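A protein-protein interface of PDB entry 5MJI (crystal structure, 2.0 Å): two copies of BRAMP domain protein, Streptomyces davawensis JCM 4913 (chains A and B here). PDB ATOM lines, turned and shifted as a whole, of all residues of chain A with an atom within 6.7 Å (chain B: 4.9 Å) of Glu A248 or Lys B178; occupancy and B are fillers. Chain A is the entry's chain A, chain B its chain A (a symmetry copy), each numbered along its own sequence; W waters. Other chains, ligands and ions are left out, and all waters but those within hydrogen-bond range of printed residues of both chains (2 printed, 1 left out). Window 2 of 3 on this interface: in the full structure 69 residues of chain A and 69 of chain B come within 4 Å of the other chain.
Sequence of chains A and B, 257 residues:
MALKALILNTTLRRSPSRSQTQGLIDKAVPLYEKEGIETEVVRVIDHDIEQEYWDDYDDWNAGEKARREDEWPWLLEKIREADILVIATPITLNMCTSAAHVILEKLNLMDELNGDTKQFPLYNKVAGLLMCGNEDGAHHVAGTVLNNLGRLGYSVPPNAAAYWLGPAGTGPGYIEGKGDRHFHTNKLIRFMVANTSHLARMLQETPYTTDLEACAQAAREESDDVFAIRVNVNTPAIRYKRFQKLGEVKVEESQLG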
ATOM      1  N   ASP A 224      20.663   8.800 -26.496  1.00  0.00           N
ATOM      2  CA  ASP A 224      21.052   8.972 -27.891  1.00  0.00           C
ATOM      3  C   ASP A 224      19.838   8.830 -28.812  1.00  0.00           C
ATOM      4  O   ASP A 224      18.802   8.279 -28.430  1.00  0.00           O
ATOM      5  CB  ASP A 224      22.100   7.926 -28.303  1.00  0.00           C
ATOM      6  CG  ASP A 224      23.317   7.913 -27.409  1.00  0.00           C
ATOM      7  OD1 ASP A 224      23.689   8.986 -26.880  1.00  0.00           O
ATOM      8  OD2 ASP A 224      23.904   6.812 -27.237  1.00  0.00           O
ATOM      9  N   VAL A 226      20.344   7.290 -31.861  1.00  0.00           N
ATOM     10  CA  VAL A 226      20.780   6.224 -32.754  1.00  0.00           C
ATOM     11  C   VAL A 226      21.083   5.017 -31.883  1.00  0.00           C
ATOM     12  O   VAL A 226      21.721   5.155 -30.834  1.00  0.00           O
ATOM     13  CB  VAL A 226      22.031   6.612 -33.575  1.00  0.00           C
ATOM     14  CG1 VAL A 226      22.569   5.403 -34.334  1.00  0.00           C
ATOM     15  CG2 VAL A 226      21.721   7.728 -34.550  1.00  0.00           C
ATOM     16  N   PHE A 227      20.619   3.843 -32.297  1.00  0.00           N
ATOM     17  CA  PHE A 227      21.044   2.590 -31.691  1.00  0.00           C
ATOM     18  C   PHE A 227      21.992   1.888 -32.654  1.00  0.00           C
ATOM     19  O   PHE A 227      21.667   1.720 -33.834  1.00  0.00           O
ATOM     20  CB  PHE A 227      19.847   1.691 -31.361  1.00  0.00           C
ATOM     21  CG  PHE A 227      20.237   0.346 -30.795  1.00  0.00           C
ATOM     22  CD1 PHE A 227      20.543  -0.719 -31.637  1.00  0.00           C
ATOM     23  CD2 PHE A 227      20.298   0.143 -29.429  1.00  0.00           C
ATOM     24  CE1 PHE A 227      20.916  -1.962 -31.127  1.00  0.00           C
ATOM     25  CE2 PHE A 227      20.660  -1.103 -28.912  1.00  0.00           C
ATOM     26  CZ  PHE A 227      20.971  -2.155 -29.772  1.00  0.00           C
ATOM     27  N   ALA A 228      23.149   1.452 -32.150  1.00  0.00           N
ATOM     28  CA  ALA A 228      24.138   0.812 -33.010  1.00  0.00           C
ATOM     29  C   ALA A 228      24.994  -0.144 -32.196  1.00  0.00           C
ATOM     30  O   ALA A 228      25.506   0.232 -31.141  1.00  0.00           O
ATOM     31  CB  ALA A 228      25.026   1.858 -33.697  1.00  0.00           C
ATOM     32  N   ILE A 229      25.136  -1.379 -32.682  1.00  0.00           N
ATOM     33  CA  ILE A 229      26.033  -2.362 -32.086  1.00  0.00           C
ATOM     34  C   ILE A 229      26.732  -3.120 -33.206  1.00  0.00           C
ATOM     35  O   ILE A 229      26.170  -3.327 -34.287  1.00  0.00           O
ATOM     36  CB  ILE A 229      25.311  -3.372 -31.147  1.00  0.00           C
ATOM     37  CG1 ILE A 229      24.103  -4.005 -31.838  1.00  0.00           C
ATOM     38  CG2 ILE A 229      24.900  -2.740 -29.828  1.00  0.00           C
ATOM     39  CD1 ILE A 229      23.635  -5.284 -31.122  1.00  0.00           C
ATOM     40  N   ARG A 230      27.963  -3.543 -32.934  1.00  0.00           N
ATOM     41  CA  ARG A 230      28.651  -4.448 -33.842  1.00  0.00           C
ATOM     42  C   ARG A 230      28.137  -5.864 -33.651  1.00  0.00           C
ATOM     43  O   ARG A 230      27.661  -6.238 -32.578  1.00  0.00           O
ATOM     44  CB  ARG A 230      30.160  -4.431 -33.620  1.00  0.00           C
ATOM     45  CG  ARG A 230      30.787  -3.087 -33.875  1.00  0.00           C
ATOM     46  CD  ARG A 230      32.280  -3.185 -34.085  1.00  0.00           C
ATOM     47  NE  ARG A 230      32.885  -1.864 -33.995  1.00  0.00           N
ATOM     48  CZ  ARG A 230      32.912  -0.980 -34.990  1.00  0.00           C
ATOM     49  NH1 ARG A 230      32.371  -1.280 -36.170  1.00  0.00           N
ATOM     50  NH2 ARG A 230      33.483   0.208 -34.801  1.00  0.00           N
ATOM     51  N   LEU A 246      33.431  -6.320 -28.977  1.00  0.00           N
ATOM     52  CA  LEU A 246      33.632  -6.026 -30.391  1.00  0.00           C
ATOM     53  C   LEU A 246      33.994  -4.567 -30.651  1.00  0.00           C
ATOM     54  O   LEU A 246      34.420  -4.238 -31.764  1.00  0.00           O
ATOM     55  CB  LEU A 246      32.372  -6.386 -31.190  1.00  0.00           C
ATOM     56  CG  LEU A 246      31.896  -7.841 -31.043  1.00  0.00           C
ATOM     57  CD1 LEU A 246      30.548  -8.054 -31.737  1.00  0.00           C
ATOM     58  CD2 LEU A 246      32.948  -8.822 -31.577  1.00  0.00           C
ATOM     59  N   GLY A 247      33.821  -3.695 -29.670  1.00  0.00           N
ATOM     60  CA  GLY A 247      34.074  -2.276 -29.848  1.00  0.00           C
ATOM     61  C   GLY A 247      32.814  -1.505 -30.179  1.00  0.00           C
ATOM     62  O   GLY A 247      31.850  -2.029 -30.733  1.00  0.00           O
ATOM     63  N   GLU A 248      32.830  -0.226 -29.843  1.00  0.00           N
ATOM     64  CA  GLU A 248      31.666   0.595 -30.107  1.00  0.00           C
ATOM     65  C   GLU A 248      31.624   1.016 -31.573  1.00  0.00           C
ATOM     66  O   GLU A 248      32.608   0.927 -32.311  1.00  0.00           O
ATOM     67  CB  GLU A 248      31.653   1.822 -29.200  1.00  0.00           C
ATOM     68  CG  GLU A 248      32.694   2.862 -29.550  1.00  0.00           C
ATOM     69  CD  GLU A 248      32.455   4.174 -28.819  1.00  0.00           C
ATOM     70  OE1 GLU A 248      31.645   4.182 -27.863  1.00  0.00           O
ATOM     71  OE2 GLU A 248      33.078   5.190 -29.201  1.00  0.00           O
ATOM     72  N   VAL A 249      30.450   1.465 -31.990  1.00  0.00           N
ATOM     73  CA  VAL A 249      30.190   1.889 -33.359  1.00  0.00           C
ATOM     74  C   VAL A 249      30.219   3.407 -33.370  1.00  0.00           C
ATOM     75  O   VAL A 249      29.517   4.046 -32.582  1.00  0.00           O
ATOM     76  CB  VAL A 249      28.827   1.372 -33.844  1.00  0.00           C
ATOM     77  CG1 VAL A 249      28.442   2.036 -35.138  1.00  0.00           C
ATOM     78  CG2 VAL A 249      28.850  -0.138 -33.985  1.00  0.00           C
ATOM     79  N   LYS A 250      31.023   4.015 -34.225  1.00  0.00           N
ATOM     80  CA  LYS A 250      31.022   5.466 -34.243  1.00  0.00           C
ATOM     81  C   LYS A 250      30.259   5.849 -35.504  1.00  0.00           C
ATOM     82  O   LYS A 250      30.442   5.246 -36.573  1.00  0.00           O
ATOM     83  CB  LYS A 250      32.451   6.032 -34.101  1.00  0.00           C
ATOM     84  CG  LYS A 250      32.746   7.584 -34.023  1.00  0.00           C
ATOM     85  CD  LYS A 250      32.975   8.202 -35.392  1.00  0.00           C
ATOM     86  CE  LYS A 250      34.276   8.151 -36.046  1.00  0.00           C
ATOM     87  NZ  LYS A 250      35.305   9.037 -35.692  1.00  0.00           N
ATOM     88  N   GLY B 173      24.782  -7.234 -24.284  1.00  0.00           N
ATOM     89  CA  GLY B 173      23.752  -6.733 -23.408  1.00  0.00           C
ATOM     90  C   GLY B 173      23.749  -5.223 -23.251  1.00  0.00           C
ATOM     91  O   GLY B 173      24.394  -4.472 -23.988  1.00  0.00           O
ATOM     92  N   TYR B 174      23.005  -4.799 -22.231  1.00  0.00           N
ATOM     93  CA  TYR B 174      22.756  -3.400 -21.895  1.00  0.00           C
ATOM     94  C   TYR B 174      24.033  -2.563 -21.800  1.00  0.00           C
ATOM     95  O   TYR B 174      24.042  -1.393 -22.198  1.00  0.00           O
ATOM     96  CB  TYR B 174      21.997  -3.380 -20.569  1.00  0.00           C
ATOM     97  CG  TYR B 174      21.636  -2.031 -19.990  1.00  0.00           C
ATOM     98  CD1 TYR B 174      22.505  -1.348 -19.135  1.00  0.00           C
ATOM     99  CD2 TYR B 174      20.403  -1.466 -20.255  1.00  0.00           C
ATOM    100  CE1 TYR B 174      22.145  -0.100 -18.584  1.00  0.00           C
ATOM    101  CE2 TYR B 174      20.037  -0.239 -19.712  1.00  0.00           C
ATOM    102  CZ  TYR B 174      20.906   0.435 -18.878  1.00  0.00           C
ATOM    103  OH  TYR B 174      20.517   1.649 -18.352  1.00  0.00           O
ATOM    104  N   ILE B 175      25.105  -3.118 -21.229  1.00  0.00           N
ATOM    105  CA  ILE B 175      26.303  -2.310 -20.975  1.00  0.00           C
ATOM    106  C   ILE B 175      27.025  -2.008 -22.288  1.00  0.00           C
ATOM    107  O   ILE B 175      27.141  -0.849 -22.697  1.00  0.00           O
ATOM    108  CB  ILE B 175      27.230  -3.003 -19.957  1.00  0.00           C
ATOM    109  CG1 ILE B 175      26.542  -3.112 -18.592  1.00  0.00           C
ATOM    110  CG2 ILE B 175      28.559  -2.223 -19.812  1.00  0.00           C
ATOM    111  CD1 ILE B 175      27.338  -3.905 -17.551  1.00  0.00           C
ATOM    112  N   GLU B 176      27.477  -3.045 -22.996  1.00  0.00           N
ATOM    113  CA  GLU B 176      28.126  -2.807 -24.287  1.00  0.00           C
ATOM    114  C   GLU B 176      27.171  -2.207 -25.316  1.00  0.00           C
ATOM    115  O   GLU B 176      27.613  -1.472 -26.203  1.00  0.00           O
ATOM    116  CB  GLU B 176      28.726  -4.102 -24.831  1.00  0.00           C
ATOM    117  CG  GLU B 176      30.025  -4.507 -24.123  1.00  0.00           C
ATOM    118  CD  GLU B 176      30.648  -5.754 -24.716  1.00  0.00           C
ATOM    119  OE1 GLU B 176      30.021  -6.376 -25.610  1.00  0.00           O
ATOM    120  OE2 GLU B 176      31.764  -6.124 -24.270  1.00  0.00           O
ATOM    121  N   GLY B 177      25.875  -2.516 -25.231  1.00  0.00           N
ATOM    122  CA  GLY B 177      24.895  -1.935 -26.131  1.00  0.00           C
ATOM    123  C   GLY B 177      24.472  -0.515 -25.803  1.00  0.00           C
ATOM    124  O   GLY B 177      23.595   0.033 -26.477  1.00  0.00           O
ATOM    125  N   LYS B 178      25.071   0.086 -24.770  1.00  0.00           N
ATOM    126  CA  LYS B 178      24.808   1.475 -24.376  1.00  0.00           C
ATOM    127  C   LYS B 178      23.350   1.680 -23.980  1.00  0.00           C
ATOM    128  O   LYS B 178      22.746   2.713 -24.278  1.00  0.00           O
ATOM    129  CB  LYS B 178      25.229   2.457 -25.478  1.00  0.00           C
ATOM    130  CG  LYS B 178      26.634   2.156 -26.000  1.00  0.00           C
ATOM    131  CD  LYS B 178      27.379   3.390 -26.453  1.00  0.00           C
ATOM    132  CE  LYS B 178      27.206   3.630 -27.942  1.00  0.00           C
ATOM    133  NZ  LYS B 178      28.371   4.373 -28.525  1.00  0.00           N
ATOM    134  N   GLY B 179      22.797   0.701 -23.259  1.00  0.00           N
ATOM    135  CA  GLY B 179      21.413   0.791 -22.827  1.00  0.00           C
ATOM    136  C   GLY B 179      21.123   1.974 -21.923  1.00  0.00           C
ATOM    137  O   GLY B 179      19.979   2.436 -21.851  1.00  0.00           O
ATOM    138  N   ASP B 180      22.140   2.482 -21.217  1.00  0.00           N
ATOM    139  CA  ASP B 180      21.904   3.617 -20.328  1.00  0.00           C
ATOM    140  C   ASP B 180      21.555   4.885 -21.093  1.00  0.00           C
ATOM    141  O   ASP B 180      20.955   5.800 -20.516  1.00  0.00           O
ATOM    142  CB  ASP B 180      23.108   3.863 -19.412  1.00  0.00           C
ATOM    143  CG  ASP B 180      24.357   4.260 -20.171  1.00  0.00           C
ATOM    144  OD1 ASP B 180      24.748   3.507 -21.093  1.00  0.00           O
ATOM    145  OD2 ASP B 180      24.942   5.327 -19.851  1.00  0.00           O
ATOM    146  N   ARG B 181      21.879   4.951 -22.381  1.00  0.00           N
ATOM    147  CA  ARG B 181      21.459   6.060 -23.225  1.00  0.00           C
ATOM    148  C   ARG B 181      20.393   5.635 -24.233  1.00  0.00           C
ATOM    149  O   ARG B 181      20.225   6.286 -25.273  1.00  0.00           O
ATOM    150  CB  ARG B 181      22.679   6.672 -23.918  1.00  0.00           C
ATOM    151  CG  ARG B 181      23.658   7.292 -22.898  1.00  0.00           C
ATOM    152  CD  ARG B 181      24.763   8.119 -23.549  1.00  0.00           C
ATOM    153  NE  ARG B 181      24.222   9.194 -24.379  1.00  0.00           N
ATOM    154  CZ  ARG B 181      23.736  10.337 -23.903  1.00  0.00           C
ATOM    155  NH1 ARG B 181      23.257  11.250 -24.739  1.00  0.00           N
ATOM    156  NH2 ARG B 181      23.727  10.573 -22.599  1.00  0.00           N
ATOM    157  N   HIS B 182      19.668   4.547 -23.952  1.00  0.00           N
ATOM    158  CA  HIS B 182      18.661   4.049 -24.881  1.00  0.00           C
ATOM    159  C   HIS B 182      17.343   4.744 -24.572  1.00  0.00           C
ATOM    160  O   HIS B 182      16.788   4.585 -23.480  1.00  0.00           O
ATOM    161  CB  HIS B 182      18.517   2.533 -24.794  1.00  0.00           C
ATOM    162  CG  HIS B 182      17.769   1.941 -25.947  1.00  0.00           C
ATOM    163  ND1 HIS B 182      16.616   1.199 -25.791  1.00  0.00           N
ATOM    164  CD2 HIS B 182      18.002   1.999 -27.280  1.00  0.00           C
ATOM    165  CE1 HIS B 182      16.176   0.819 -26.979  1.00  0.00           C
ATOM    166  NE2 HIS B 182      16.996   1.292 -27.898  1.00  0.00           N
HETATM  167  O   HOH W   1      30.504  -5.800 -28.231  1.00  0.00           O
HETATM  168  O   HOH W   2      28.128   1.634 -30.297  1.00  0.00           O
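No position is printed for both chains. Of the 5 pairs that touch across the chains among the printed residues, none has its exchanged pair printed and touching as well.
Printed residues of chain B that touch a printed residue of chain A: Gly B177, Lys B178, Arg B181 and His B182. Hydrophobic or aromatic side chains of chain B within 4 Å of the printed part of chain A: His B182. Hydrophobic or aromatic side chains of chain A within 4 Å of the printed part of chain B: Phe A227 and Ile A229. Among the printed residues, Asp or Glu carboxylates within 4 Å of a Lys or Arg side-chain nitrogen of the other chain: Asp A224 with Arg B181 and Glu A248 with Lys B178.
Water W1 lies within hydrogen-bond range of OE1 of Glu B176 (2.7 Å) and N of Leu A246 (3.1 Å). Water W2 lies within hydrogen-bond range of the backbone NH (N) of Val A249 (2.9 Å), the backbone carbonyl oxygen (O) of Ala A228 (3.1 Å) and the side-chain amino group (NZ) of Lys B178 (3.3 Å).
Among the printed residues, pairs that only touch across the chains: Phe A227 with His B182 (3.7 Å), Ile A229 with Gly B177 (3.8 Å) and Phe A227 with Gly B177 (3.98 Å).
Glu A248 touches one residue of chain B. Of chain A, only Glu A248 comes within 4 Å of Lys B178. Of the printed residues of chain A, His B182 touches Phe A227. Of the printed residues of chain A, Arg B181 touches Asp A224 (2.6 Å). Of the printed residues of chain B, Asp A224 touches Arg B181. The nearest printed residue of chain B that does not touch Glu A248 is Glu B176 (6.0 Å). The nearest printed residue of chain B that does not touch Ile A229 is Glu B176 (4.7 Å).
The guanidinium group (NH2) of Arg A230 lies within hydrogen-bond range of the backbone carbonyl oxygen (O) of Glu A248 (2.7 Å).
The side-chain carboxylate (OD1) of Asp A224 is in salt-bridge range of the guanidinium group (NE) of Arg B181, 2.6 Å away. The side-chain carboxylate (OE1) of Glu A248 lies within salt-bridge range of the side-chain amino group (NZ) of Lys B178, 3.3 Å away.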
